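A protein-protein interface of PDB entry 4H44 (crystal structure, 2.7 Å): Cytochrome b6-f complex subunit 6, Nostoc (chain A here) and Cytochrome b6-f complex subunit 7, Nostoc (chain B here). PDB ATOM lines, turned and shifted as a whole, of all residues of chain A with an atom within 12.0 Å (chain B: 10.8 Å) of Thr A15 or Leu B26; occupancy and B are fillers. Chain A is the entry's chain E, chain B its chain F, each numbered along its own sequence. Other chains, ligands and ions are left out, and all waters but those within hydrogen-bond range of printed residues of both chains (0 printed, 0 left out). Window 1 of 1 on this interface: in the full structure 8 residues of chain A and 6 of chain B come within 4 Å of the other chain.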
ATOM      1  N   VAL A   5     -34.881  13.346 -16.679  1.00  0.00           N
ATOM      2  CA  VAL A   5     -34.472  13.503 -15.289  1.00  0.00           C
ATOM      3  C   VAL A   5     -34.731  12.219 -14.501  1.00  0.00           C
ATOM      4  O   VAL A   5     -33.928  11.826 -13.652  1.00  0.00           O
ATOM      5  CB  VAL A   5     -35.223  14.668 -14.616  1.00  0.00           C
ATOM      6  CG1 VAL A   5     -34.968  14.673 -13.115  1.00  0.00           C
ATOM      7  CG2 VAL A   5     -34.809  15.994 -15.237  1.00  0.00           C
ATOM      8  N   ALA A   6     -35.854  11.573 -14.790  1.00  0.00           N
ATOM      9  CA  ALA A   6     -36.235  10.347 -14.099  1.00  0.00           C
ATOM     10  C   ALA A   6     -35.307   9.196 -14.474  1.00  0.00           C
ATOM     11  O   ALA A   6     -34.893   8.418 -13.618  1.00  0.00           O
ATOM     12  CB  ALA A   6     -37.672   9.989 -14.426  1.00  0.00           C
ATOM     13  N   TYR A   7     -34.989   9.098 -15.760  1.00  0.00           N
ATOM     14  CA  TYR A   7     -34.109   8.046 -16.257  1.00  0.00           C
ATOM     15  C   TYR A   7     -32.716   8.154 -15.637  1.00  0.00           C
ATOM     16  O   TYR A   7     -32.189   7.177 -15.102  1.00  0.00           O
ATOM     17  CB  TYR A   7     -34.011   8.128 -17.782  1.00  0.00           C
ATOM     18  CG  TYR A   7     -32.999   7.180 -18.383  1.00  0.00           C
ATOM     19  CD1 TYR A   7     -33.333   5.861 -18.663  1.00  0.00           C
ATOM     20  CD2 TYR A   7     -31.712   7.608 -18.676  1.00  0.00           C
ATOM     21  CE1 TYR A   7     -32.408   4.992 -19.214  1.00  0.00           C
ATOM     22  CE2 TYR A   7     -30.783   6.749 -19.227  1.00  0.00           C
ATOM     23  CZ  TYR A   7     -31.135   5.443 -19.499  1.00  0.00           C
ATOM     24  OH  TYR A   7     -30.201   4.591 -20.042  1.00  0.00           O
ATOM     25  N   ILE A   8     -32.133   9.347 -15.709  1.00  0.00           N
ATOM     26  CA  ILE A   8     -30.799   9.589 -15.170  1.00  0.00           C
ATOM     27  C   ILE A   8     -30.779   9.439 -13.651  1.00  0.00           C
ATOM     28  O   ILE A   8     -29.786   8.990 -13.077  1.00  0.00           O
ATOM     29  CB  ILE A   8     -30.299  11.002 -15.529  1.00  0.00           C
ATOM     30  CG1 ILE A   8     -30.168  11.152 -17.047  1.00  0.00           C
ATOM     31  CG2 ILE A   8     -28.963  11.279 -14.852  1.00  0.00           C
ATOM     32  CD1 ILE A   8     -29.722  12.527 -17.493  1.00  0.00           C
ATOM     33  N   GLY A   9     -31.876   9.822 -13.004  1.00  0.00           N
ATOM     34  CA  GLY A   9     -31.972   9.742 -11.558  1.00  0.00           C
ATOM     35  C   GLY A   9     -32.196   8.327 -11.058  1.00  0.00           C
ATOM     36  O   GLY A   9     -31.791   7.977  -9.949  1.00  0.00           O
ATOM     37  N   PHE A  10     -32.843   7.512 -11.885  1.00  0.00           N
ATOM     38  CA  PHE A  10     -33.136   6.130 -11.534  1.00  0.00           C
ATOM     39  C   PHE A  10     -31.844   5.330 -11.628  1.00  0.00           C
ATOM     40  O   PHE A  10     -31.485   4.587 -10.711  1.00  0.00           O
ATOM     41  CB  PHE A  10     -34.186   5.564 -12.494  1.00  0.00           C
ATOM     42  CG  PHE A  10     -35.095   4.531 -11.878  1.00  0.00           C
ATOM     43  CD1 PHE A  10     -36.306   4.219 -12.481  1.00  0.00           C
ATOM     44  CD2 PHE A  10     -34.748   3.874 -10.710  1.00  0.00           C
ATOM     45  CE1 PHE A  10     -37.152   3.274 -11.931  1.00  0.00           C
ATOM     46  CE2 PHE A  10     -35.594   2.928 -10.156  1.00  0.00           C
ATOM     47  CZ  PHE A  10     -36.796   2.628 -10.767  1.00  0.00           C
ATOM     48  N   LEU A  11     -31.142   5.504 -12.744  1.00  0.00           N
ATOM     49  CA  LEU A  11     -29.865   4.838 -12.962  1.00  0.00           C
ATOM     50  C   LEU A  11     -28.809   5.317 -11.973  1.00  0.00           C
ATOM     51  O   LEU A  11     -27.977   4.535 -11.519  1.00  0.00           O
ATOM     52  CB  LEU A  11     -29.371   5.087 -14.385  1.00  0.00           C
ATOM     53  CG  LEU A  11     -30.187   4.445 -15.504  1.00  0.00           C
ATOM     54  CD1 LEU A  11     -29.599   4.814 -16.848  1.00  0.00           C
ATOM     55  CD2 LEU A  11     -30.239   2.934 -15.339  1.00  0.00           C
ATOM     56  N   ALA A  12     -28.836   6.608 -11.657  1.00  0.00           N
ATOM     57  CA  ALA A  12     -27.878   7.185 -10.724  1.00  0.00           C
ATOM     58  C   ALA A  12     -28.130   6.630  -9.330  1.00  0.00           C
ATOM     59  O   ALA A  12     -27.195   6.324  -8.588  1.00  0.00           O
ATOM     60  CB  ALA A  12     -27.996   8.696 -10.715  1.00  0.00           C
ATOM     61  N   LEU A  13     -29.407   6.501  -8.988  1.00  0.00           N
ATOM     62  CA  LEU A  13     -29.799   5.969  -7.692  1.00  0.00           C
ATOM     63  C   LEU A  13     -29.297   4.540  -7.521  1.00  0.00           C
ATOM     64  O   LEU A  13     -28.677   4.214  -6.508  1.00  0.00           O
ATOM     65  CB  LEU A  13     -31.320   6.014  -7.543  1.00  0.00           C
ATOM     66  CG  LEU A  13     -31.891   5.285  -6.326  1.00  0.00           C
ATOM     67  CD1 LEU A  13     -31.356   5.884  -5.035  1.00  0.00           C
ATOM     68  CD2 LEU A  13     -33.412   5.320  -6.349  1.00  0.00           C
ATOM     69  N   PHE A  14     -29.560   3.694  -8.513  1.00  0.00           N
ATOM     70  CA  PHE A  14     -29.179   2.285  -8.432  1.00  0.00           C
ATOM     71  C   PHE A  14     -27.683   2.059  -8.652  1.00  0.00           C
ATOM     72  O   PHE A  14     -27.135   1.036  -8.239  1.00  0.00           O
ATOM     73  CB  PHE A  14     -29.997   1.445  -9.414  1.00  0.00           C
ATOM     74  CG  PHE A  14     -31.179   0.774  -8.785  1.00  0.00           C
ATOM     75  CD1 PHE A  14     -32.401   1.419  -8.709  1.00  0.00           C
ATOM     76  CD2 PHE A  14     -31.062  -0.499  -8.254  1.00  0.00           C
ATOM     77  CE1 PHE A  14     -33.487   0.799  -8.121  1.00  0.00           C
ATOM     78  CE2 PHE A  14     -32.145  -1.120  -7.665  1.00  0.00           C
ATOM     79  CZ  PHE A  14     -33.359  -0.470  -7.599  1.00  0.00           C
ATOM     80  N   THR A  15     -27.022   3.013  -9.300  1.00  0.00           N
ATOM     81  CA  THR A  15     -25.573   2.955  -9.447  1.00  0.00           C
ATOM     82  C   THR A  15     -24.964   3.304  -8.100  1.00  0.00           C
ATOM     83  O   THR A  15     -23.894   2.810  -7.735  1.00  0.00           O
ATOM     84  CB  THR A  15     -25.064   3.936 -10.519  1.00  0.00           C
ATOM     85  OG1 THR A  15     -25.513   3.513 -11.814  1.00  0.00           O
ATOM     86  CG2 THR A  15     -23.543   3.993 -10.514  1.00  0.00           C
ATOM     87  N   GLY A  16     -25.664   4.161  -7.362  1.00  0.00           N
ATOM     88  CA  GLY A  16     -25.262   4.523  -6.016  1.00  0.00           C
ATOM     89  C   GLY A  16     -25.578   3.417  -5.027  1.00  0.00           C
ATOM     90  O   GLY A  16     -24.888   3.256  -4.021  1.00  0.00           O
ATOM     91  N   ILE A  17     -26.630   2.656  -5.310  1.00  0.00           N
ATOM     92  CA  ILE A  17     -26.972   1.496  -4.493  1.00  0.00           C
ATOM     93  C   ILE A  17     -25.981   0.368  -4.760  1.00  0.00           C
ATOM     94  O   ILE A  17     -25.669  -0.422  -3.869  1.00  0.00           O
ATOM     95  CB  ILE A  17     -28.400   0.991  -4.781  1.00  0.00           C
ATOM     96  CG1 ILE A  17     -29.437   2.007  -4.295  1.00  0.00           C
ATOM     97  CG2 ILE A  17     -28.634  -0.344  -4.095  1.00  0.00           C
ATOM     98  CD1 ILE A  17     -30.861   1.673  -4.695  1.00  0.00           C
ATOM     99  N   ALA A  18     -25.489   0.295  -5.992  1.00  0.00           N
ATOM    100  CA  ALA A  18     -24.518  -0.729  -6.362  1.00  0.00           C
ATOM    101  C   ALA A  18     -23.182  -0.472  -5.670  1.00  0.00           C
ATOM    102  O   ALA A  18     -22.624  -1.361  -5.024  1.00  0.00           O
ATOM    103  CB  ALA A  18     -24.336  -0.759  -7.866  1.00  0.00           C
ATOM    104  N   ALA A  19     -22.676   0.750  -5.813  1.00  0.00           N
ATOM    105  CA  ALA A  19     -21.424   1.143  -5.178  1.00  0.00           C
ATOM    106  C   ALA A  19     -21.549   1.052  -3.661  1.00  0.00           C
ATOM    107  O   ALA A  19     -20.624   0.609  -2.979  1.00  0.00           O
ATOM    108  CB  ALA A  19     -21.047   2.554  -5.590  1.00  0.00           C
ATOM    109  N   GLY A  20     -22.698   1.467  -3.139  1.00  0.00           N
ATOM    110  CA  GLY A  20     -22.938   1.448  -1.708  1.00  0.00           C
ATOM    111  C   GLY A  20     -22.889   0.041  -1.150  1.00  0.00           C
ATOM    112  O   GLY A  20     -22.305  -0.198  -0.092  1.00  0.00           O
ATOM    113  N   LEU A  21     -23.507  -0.894  -1.865  1.00  0.00           N
ATOM    114  CA  LEU A  21     -23.522  -2.291  -1.449  1.00  0.00           C
ATOM    115  C   LEU A  21     -22.147  -2.919  -1.633  1.00  0.00           C
ATOM    116  O   LEU A  21     -21.768  -3.835  -0.904  1.00  0.00           O
ATOM    117  CB  LEU A  21     -24.559  -3.082  -2.252  1.00  0.00           C
ATOM    118  CG  LEU A  21     -25.938  -3.323  -1.625  1.00  0.00           C
ATOM    119  CD1 LEU A  21     -25.811  -3.999  -0.268  1.00  0.00           C
ATOM    120  CD2 LEU A  21     -26.737  -2.035  -1.510  1.00  0.00           C
ATOM    121  N   LEU A  22     -21.404  -2.421  -2.617  1.00  0.00           N
ATOM    122  CA  LEU A  22     -20.071  -2.935  -2.900  1.00  0.00           C
ATOM    123  C   LEU A  22     -19.125  -2.628  -1.745  1.00  0.00           C
ATOM    124  O   LEU A  22     -18.672  -3.534  -1.044  1.00  0.00           O
ATOM    125  CB  LEU A  22     -19.532  -2.335  -4.200  1.00  0.00           C
ATOM    126  CG  LEU A  22     -18.096  -2.720  -4.564  1.00  0.00           C
ATOM    127  CD1 LEU A  22     -17.932  -4.229  -4.599  1.00  0.00           C
ATOM    128  CD2 LEU A  22     -17.697  -2.109  -5.900  1.00  0.00           C
ATOM    129  N   PHE A  23     -18.836  -1.345  -1.550  1.00  0.00           N
ATOM    130  CA  PHE A  23     -17.941  -0.911  -0.484  1.00  0.00           C
ATOM    131  C   PHE A  23     -18.534  -1.220   0.888  1.00  0.00           C
ATOM    132  O   PHE A  23     -17.802  -1.436   1.853  1.00  0.00           O
ATOM    133  CB  PHE A  23     -17.658   0.588  -0.607  1.00  0.00           C
ATOM    134  CG  PHE A  23     -17.015   0.977  -1.909  1.00  0.00           C
ATOM    135  CD1 PHE A  23     -17.714   1.712  -2.853  1.00  0.00           C
ATOM    136  CD2 PHE A  23     -15.713   0.600  -2.193  1.00  0.00           C
ATOM    137  CE1 PHE A  23     -17.124   2.068  -4.051  1.00  0.00           C
ATOM    138  CE2 PHE A  23     -15.119   0.952  -3.391  1.00  0.00           C
ATOM    139  CZ  PHE A  23     -15.825   1.688  -4.320  1.00  0.00           C
ATOM    140  N   GLY A  24     -19.861  -1.247   0.966  1.00  0.00           N
ATOM    141  CA  GLY A  24     -20.542  -1.518   2.217  1.00  0.00           C
ATOM    142  C   GLY A  24     -20.338  -2.947   2.684  1.00  0.00           C
ATOM    143  O   GLY A  24     -20.106  -3.193   3.867  1.00  0.00           O
ATOM    144  N   LEU A  25     -20.427  -3.887   1.750  1.00  0.00           N
ATOM    145  CA  LEU A  25     -20.269  -5.301   2.071  1.00  0.00           C
ATOM    146  C   LEU A  25     -18.795  -5.658   2.219  1.00  0.00           C
ATOM    147  O   LEU A  25     -18.442  -6.583   2.950  1.00  0.00           O
ATOM    148  CB  LEU A  25     -20.921  -6.167   0.992  1.00  0.00           C
ATOM    149  CG  LEU A  25     -22.450  -6.113   0.933  1.00  0.00           C
ATOM    150  CD1 LEU A  25     -22.964  -6.835  -0.305  1.00  0.00           C
ATOM    151  CD2 LEU A  25     -23.055  -6.715   2.190  1.00  0.00           C
ATOM    152  N   ARG A  26     -17.939  -4.924   1.514  1.00  0.00           N
ATOM    153  CA  ARG A  26     -16.498  -5.075   1.669  1.00  0.00           C
ATOM    154  C   ARG A  26     -16.095  -4.752   3.101  1.00  0.00           C
ATOM    155  O   ARG A  26     -15.392  -5.527   3.752  1.00  0.00           O
ATOM    156  CB  ARG A  26     -15.755  -4.148   0.707  1.00  0.00           C
ATOM    157  CG  ARG A  26     -15.605  -4.692  -0.700  1.00  0.00           C
ATOM    158  CD  ARG A  26     -14.939  -3.672  -1.608  1.00  0.00           C
ATOM    159  NE  ARG A  26     -14.582  -4.239  -2.904  1.00  0.00           N
ATOM    160  CZ  ARG A  26     -14.114  -3.534  -3.929  1.00  0.00           C
ATOM    161  NH1 ARG A  26     -13.944  -2.223  -3.819  1.00  0.00           N
ATOM    162  NH2 ARG A  26     -13.815  -4.141  -5.068  1.00  0.00           N
ATOM    163  N   LEU A  31     -17.501  -9.205   1.337  1.00  0.00           N
ATOM    164  CA  LEU A  31     -16.879  -9.298   0.021  1.00  0.00           C
ATOM    165  C   LEU A  31     -15.361  -9.257   0.147  1.00  0.00           C
ATOM    166  O   LEU A  31     -14.711  -8.332  -0.341  1.00  0.00           O
ATOM    167  CB  LEU A  31     -17.353  -8.164  -0.889  1.00  0.00           C
ATOM    168  CG  LEU A  31     -18.836  -8.152  -1.269  1.00  0.00           C
ATOM    169  CD1 LEU A  31     -19.072  -7.175  -2.412  1.00  0.00           C
ATOM    170  CD2 LEU A  31     -19.325  -9.543  -1.640  1.00  0.00           C
ATOM    171  N   VAL B  18     -25.531   3.067 -23.064  1.00  0.00           N
ATOM    172  CA  VAL B  18     -25.629   3.611 -21.715  1.00  0.00           C
ATOM    173  C   VAL B  18     -25.419   2.507 -20.685  1.00  0.00           C
ATOM    174  O   VAL B  18     -24.757   2.714 -19.670  1.00  0.00           O
ATOM    175  CB  VAL B  18     -26.998   4.269 -21.463  1.00  0.00           C
ATOM    176  CG1 VAL B  18     -27.072   4.801 -20.041  1.00  0.00           C
ATOM    177  CG2 VAL B  18     -27.246   5.381 -22.465  1.00  0.00           C
ATOM    178  N   GLY B  19     -25.991   1.335 -20.950  1.00  0.00           N
ATOM    179  CA  GLY B  19     -25.842   0.195 -20.064  1.00  0.00           C
ATOM    180  C   GLY B  19     -24.434  -0.366 -20.129  1.00  0.00           C
ATOM    181  O   GLY B  19     -23.900  -0.869 -19.139  1.00  0.00           O
ATOM    182  N   TRP B  20     -23.830  -0.256 -21.307  1.00  0.00           N
ATOM    183  CA  TRP B  20     -22.461  -0.700 -21.516  1.00  0.00           C
ATOM    184  C   TRP B  20     -21.544   0.200 -20.705  1.00  0.00           C
ATOM    185  O   TRP B  20     -20.626  -0.270 -20.038  1.00  0.00           O
ATOM    186  CB  TRP B  20     -22.106  -0.609 -22.999  1.00  0.00           C
ATOM    187  CG  TRP B  20     -20.743  -1.143 -23.339  1.00  0.00           C
ATOM    188  CD1 TRP B  20     -19.873  -1.771 -22.496  1.00  0.00           C
ATOM    189  CD2 TRP B  20     -20.097  -1.092 -24.617  1.00  0.00           C
ATOM    190  NE1 TRP B  20     -18.726  -2.116 -23.170  1.00  0.00           N
ATOM    191  CE2 TRP B  20     -18.838  -1.709 -24.474  1.00  0.00           C
ATOM    192  CE3 TRP B  20     -20.459  -0.584 -25.869  1.00  0.00           C
ATOM    193  CZ2 TRP B  20     -17.941  -1.831 -25.532  1.00  0.00           C
ATOM    194  CZ3 TRP B  20     -19.566  -0.708 -26.920  1.00  0.00           C
ATOM    195  CH2 TRP B  20     -18.323  -1.326 -26.745  1.00  0.00           C
ATOM    196  N   ALA B  21     -21.820   1.499 -20.763  1.00  0.00           N
ATOM    197  CA  ALA B  21     -21.016   2.490 -20.063  1.00  0.00           C
ATOM    198  C   ALA B  21     -21.106   2.299 -18.555  1.00  0.00           C
ATOM    199  O   ALA B  21     -20.097   2.370 -17.855  1.00  0.00           O
ATOM    200  CB  ALA B  21     -21.469   3.885 -20.440  1.00  0.00           C
ATOM    201  N   LEU B  22     -22.317   2.066 -18.059  1.00  0.00           N
ATOM    202  CA  LEU B  22     -22.530   1.864 -16.631  1.00  0.00           C
ATOM    203  C   LEU B  22     -21.853   0.590 -16.153  1.00  0.00           C
ATOM    204  O   LEU B  22     -21.344   0.541 -15.038  1.00  0.00           O
ATOM    205  CB  LEU B  22     -24.025   1.808 -16.305  1.00  0.00           C
ATOM    206  CG  LEU B  22     -24.751   3.147 -16.155  1.00  0.00           C
ATOM    207  CD1 LEU B  22     -26.242   2.919 -15.970  1.00  0.00           C
ATOM    208  CD2 LEU B  22     -24.187   3.945 -14.988  1.00  0.00           C
ATOM    209  N   GLY B  23     -21.851  -0.443 -16.990  1.00  0.00           N
ATOM    210  CA  GLY B  23     -21.189  -1.688 -16.646  1.00  0.00           C
ATOM    211  C   GLY B  23     -19.693  -1.496 -16.500  1.00  0.00           C
ATOM    212  O   GLY B  23     -19.093  -1.923 -15.512  1.00  0.00           O
ATOM    213  N   ALA B  24     -19.095  -0.843 -17.492  1.00  0.00           N
ATOM    214  CA  ALA B  24     -17.665  -0.573 -17.492  1.00  0.00           C
ATOM    215  C   ALA B  24     -17.314   0.305 -16.301  1.00  0.00           C
ATOM    216  O   ALA B  24     -16.253   0.156 -15.695  1.00  0.00           O
ATOM    217  CB  ALA B  24     -17.259   0.110 -18.793  1.00  0.00           C
ATOM    218  N   LEU B  25     -18.226   1.210 -15.961  1.00  0.00           N
ATOM    219  CA  LEU B  25     -18.005   2.143 -14.866  1.00  0.00           C
ATOM    220  C   LEU B  25     -17.912   1.373 -13.555  1.00  0.00           C
ATOM    221  O   LEU B  25     -16.977   1.562 -12.783  1.00  0.00           O
ATOM    222  CB  LEU B  25     -19.135   3.175 -14.814  1.00  0.00           C
ATOM    223  CG  LEU B  25     -18.855   4.453 -14.017  1.00  0.00           C
ATOM    224  CD1 LEU B  25     -19.776   5.572 -14.481  1.00  0.00           C
ATOM    225  CD2 LEU B  25     -19.017   4.218 -12.524  1.00  0.00           C
ATOM    226  N   LEU B  26     -18.877   0.491 -13.321  1.00  0.00           N
ATOM    227  CA  LEU B  26     -18.896  -0.311 -12.104  1.00  0.00           C
ATOM    228  C   LEU B  26     -17.675  -1.219 -12.050  1.00  0.00           C
ATOM    229  O   LEU B  26     -17.170  -1.530 -10.971  1.00  0.00           O
ATOM    230  CB  LEU B  26     -20.177  -1.147 -12.022  1.00  0.00           C
ATOM    231  CG  LEU B  26     -21.371  -0.514 -11.298  1.00  0.00           C
ATOM    232  CD1 LEU B  26     -21.027  -0.210  -9.846  1.00  0.00           C
ATOM    233  CD2 LEU B  26     -21.844   0.741 -12.007  1.00  0.00           C
ATOM    234  N   LEU B  27     -17.205  -1.649 -13.217  1.00  0.00           N
ATOM    235  CA  LEU B  27     -15.979  -2.433 -13.295  1.00  0.00           C
ATOM    236  C   LEU B  27     -14.774  -1.620 -12.829  1.00  0.00           C
ATOM    237  O   LEU B  27     -13.904  -2.136 -12.126  1.00  0.00           O
ATOM    238  CB  LEU B  27     -15.751  -2.944 -14.718  1.00  0.00           C
ATOM    239  CG  LEU B  27     -16.600  -4.154 -15.115  1.00  0.00           C
ATOM    240  CD1 LEU B  27     -16.487  -4.427 -16.604  1.00  0.00           C
ATOM    241  CD2 LEU B  27     -16.187  -5.381 -14.316  1.00  0.00           C
ATOM    242  N   LYS B  28     -14.724  -0.352 -13.223  1.00  0.00           N
ATOM    243  CA  LYS B  28     -13.628   0.528 -12.825  1.00  0.00           C
ATOM    244  C   LYS B  28     -13.565   0.735 -11.311  1.00  0.00           C
ATOM    245  O   LYS B  28     -12.484   0.710 -10.727  1.00  0.00           O
ATOM    246  CB  LYS B  28     -13.751   1.885 -13.521  1.00  0.00           C
ATOM    247  CG  LYS B  28     -13.720   1.819 -15.041  1.00  0.00           C
ATOM    248  CD  LYS B  28     -12.411   2.355 -15.607  1.00  0.00           C
ATOM    249  CE  LYS B  28     -11.219   1.498 -15.205  1.00  0.00           C
ATOM    250  NZ  LYS B  28      -9.947   2.004 -15.792  1.00  0.00           N
ATOM    251  N   ILE B  29     -14.719   0.937 -10.676  1.00  0.00           N
ATOM    252  CA  ILE B  29     -14.741   1.298  -9.257  1.00  0.00           C
ATOM    253  C   ILE B  29     -14.470   0.100  -8.349  1.00  0.00           C
ATOM    254  O   ILE B  29     -14.083   0.271  -7.193  1.00  0.00           O
ATOM    255  CB  ILE B  29     -16.080   1.962  -8.823  1.00  0.00           C
ATOM    256  CG1 ILE B  29     -17.118   0.907  -8.429  1.00  0.00           C
ATOM    257  CG2 ILE B  29     -16.615   2.883  -9.915  1.00  0.00           C
ATOM    258  CD1 ILE B  29     -18.390   1.498  -7.854  1.00  0.00           C
ATOM    259  N   GLN B  30     -14.673  -1.108  -8.863  1.00  0.00           N
ATOM    260  CA  GLN B  30     -14.416  -2.308  -8.076  1.00  0.00           C
ATOM    261  C   GLN B  30     -12.950  -2.713  -8.174  1.00  0.00           C
ATOM    262  O   GLN B  30     -12.451  -3.472  -7.343  1.00  0.00           O
ATOM    263  CB  GLN B  30     -15.308  -3.468  -8.531  1.00  0.00           C
ATOM    264  CG  GLN B  30     -14.949  -4.050  -9.892  1.00  0.00           C
ATOM    265  CD  GLN B  30     -15.068  -5.565  -9.934  1.00  0.00           C
ATOM    266  OE1 GLN B  30     -15.309  -6.211  -8.914  1.00  0.00           O
ATOM    267  NE2 GLN B  30     -14.892  -6.139 -11.118  1.00  0.00           N
ATOM    268  N   GLY B  31     -12.264  -2.203  -9.193  1.00  0.00           N
ATOM    269  CA  GLY B  31     -10.868  -2.532  -9.410  1.00  0.00           C
ATOM    270  C   GLY B  31     -10.713  -3.778 -10.257  1.00  0.00           C
ATOM    271  O   GLY B  31     -10.271  -4.821  -9.773  1.00  0.00           O
ATOM    272  N   ALA B  32     -11.080  -3.670 -11.529  1.00  0.00           N
ATOM    273  CA  ALA B  32     -10.989  -4.795 -12.450  1.00  0.00           C
ATOM    274  C   ALA B  32      -9.529  -5.156 -12.712  1.00  0.00           C
ATOM    275  O   ALA B  32      -9.231  -6.127 -13.408  1.00  0.00           O
ATOM    276  CB  ALA B  32     -11.695  -4.464 -13.756  1.00  0.00           C
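O of Gln B30 lies within hydrogen-bond range of NH2 of Arg A26, 2.7 Å away.
The side-chain hydroxyl of Thr A15 lies within hydrogen-bond range of the backbone carbonyl oxygen of Leu A11, 2.7 Å away.
Among the printed residues, merely in contact across the chains: Tyr A7 with Val B18 (3.1 Å), Thr A15 with Leu B22 (3.5 Å), Phe A23 with Ile B29 (3.6 Å), Ala A19 with Ile B29 (3.6 Å), Leu A22 with Gln B30 (3.8 Å), Ala A18 with Leu B26 (3.9 Å), Leu A11 with Leu B22 (3.95 Å), Thr A15 with Leu B26 (3.96 Å) and Leu A22 with Ile B29 (3.98 Å).
Of the printed residues of chain B, Tyr A7 touches Val B18 (3.1 Å). No residue of chain B comes within 4 Å of Ala A12. Thr A15 touches just these residues of chain B: Leu B22 (3.5 Å) and Leu B26 (3.96 Å). No residue of chain B comes within 4 Å of Gly A16. Ala A18 touches just one residue of chain B: Leu B26. Ala A19 touches just one residue of chain B: Ile B29. Of the printed residues of chain B, Leu A22 touches Ile B29 and Gln B30. Of the printed residues of chain B, Phe A23 touches Ile B29. Of the printed residues of chain B, Arg A26 touches Gln B30. Printed residues of chain A within 4 Å of Val B18: Tyr A7 (3.1 Å). No residue of chain A comes within 4 Å of Gly B23. Ala B24 touches none of the printed residues of chain A. No residue of chain A comes within 4 Å of Leu B25. Leu B26 touches two residues of chain A. No residue of chain A comes within 4 Å of Leu B27. Ile B29 touches just these residues of chain A: Ala A19 (3.6 Å), Leu A22 (3.98 Å) and Phe A23 (3.6 Å). Gln B30 touches just these residues of chain A: Leu A22 (3.8 Å) and Arg A26 (2.7 Å). No residue of chain A comes within 4 Å of Gly B31. The nearest residue of chain A that does not touch Leu B26 is Ala A19 (4.5 Å). The nearest printed residue of chain B that does not touch Leu A22 is Leu B26 (5.1 Å).
Of the 15 printed residues of chain B, 5 touch a printed residue of chain A. Hydrophobic or aromatic side chains of chain B that line the printed part of chain A: Val B18, Leu B22, Leu B26 and Ile B29. Of the 23 printed residues of chain A, 8 touch a printed residue of chain B. Hydrophobic or aromatic side chains of chain A within 4 Å of the printed part of chain B: Tyr A7, Leu A11, Ala A18, Ala A19, Leu A22 and Phe A23. Among the printed residues, 10 pairs touch across the chains. Among the printed residues, no Asp or Glu carboxylate lies within 4 Å of a Lys or Arg side-chain nitrogen of the other chain.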
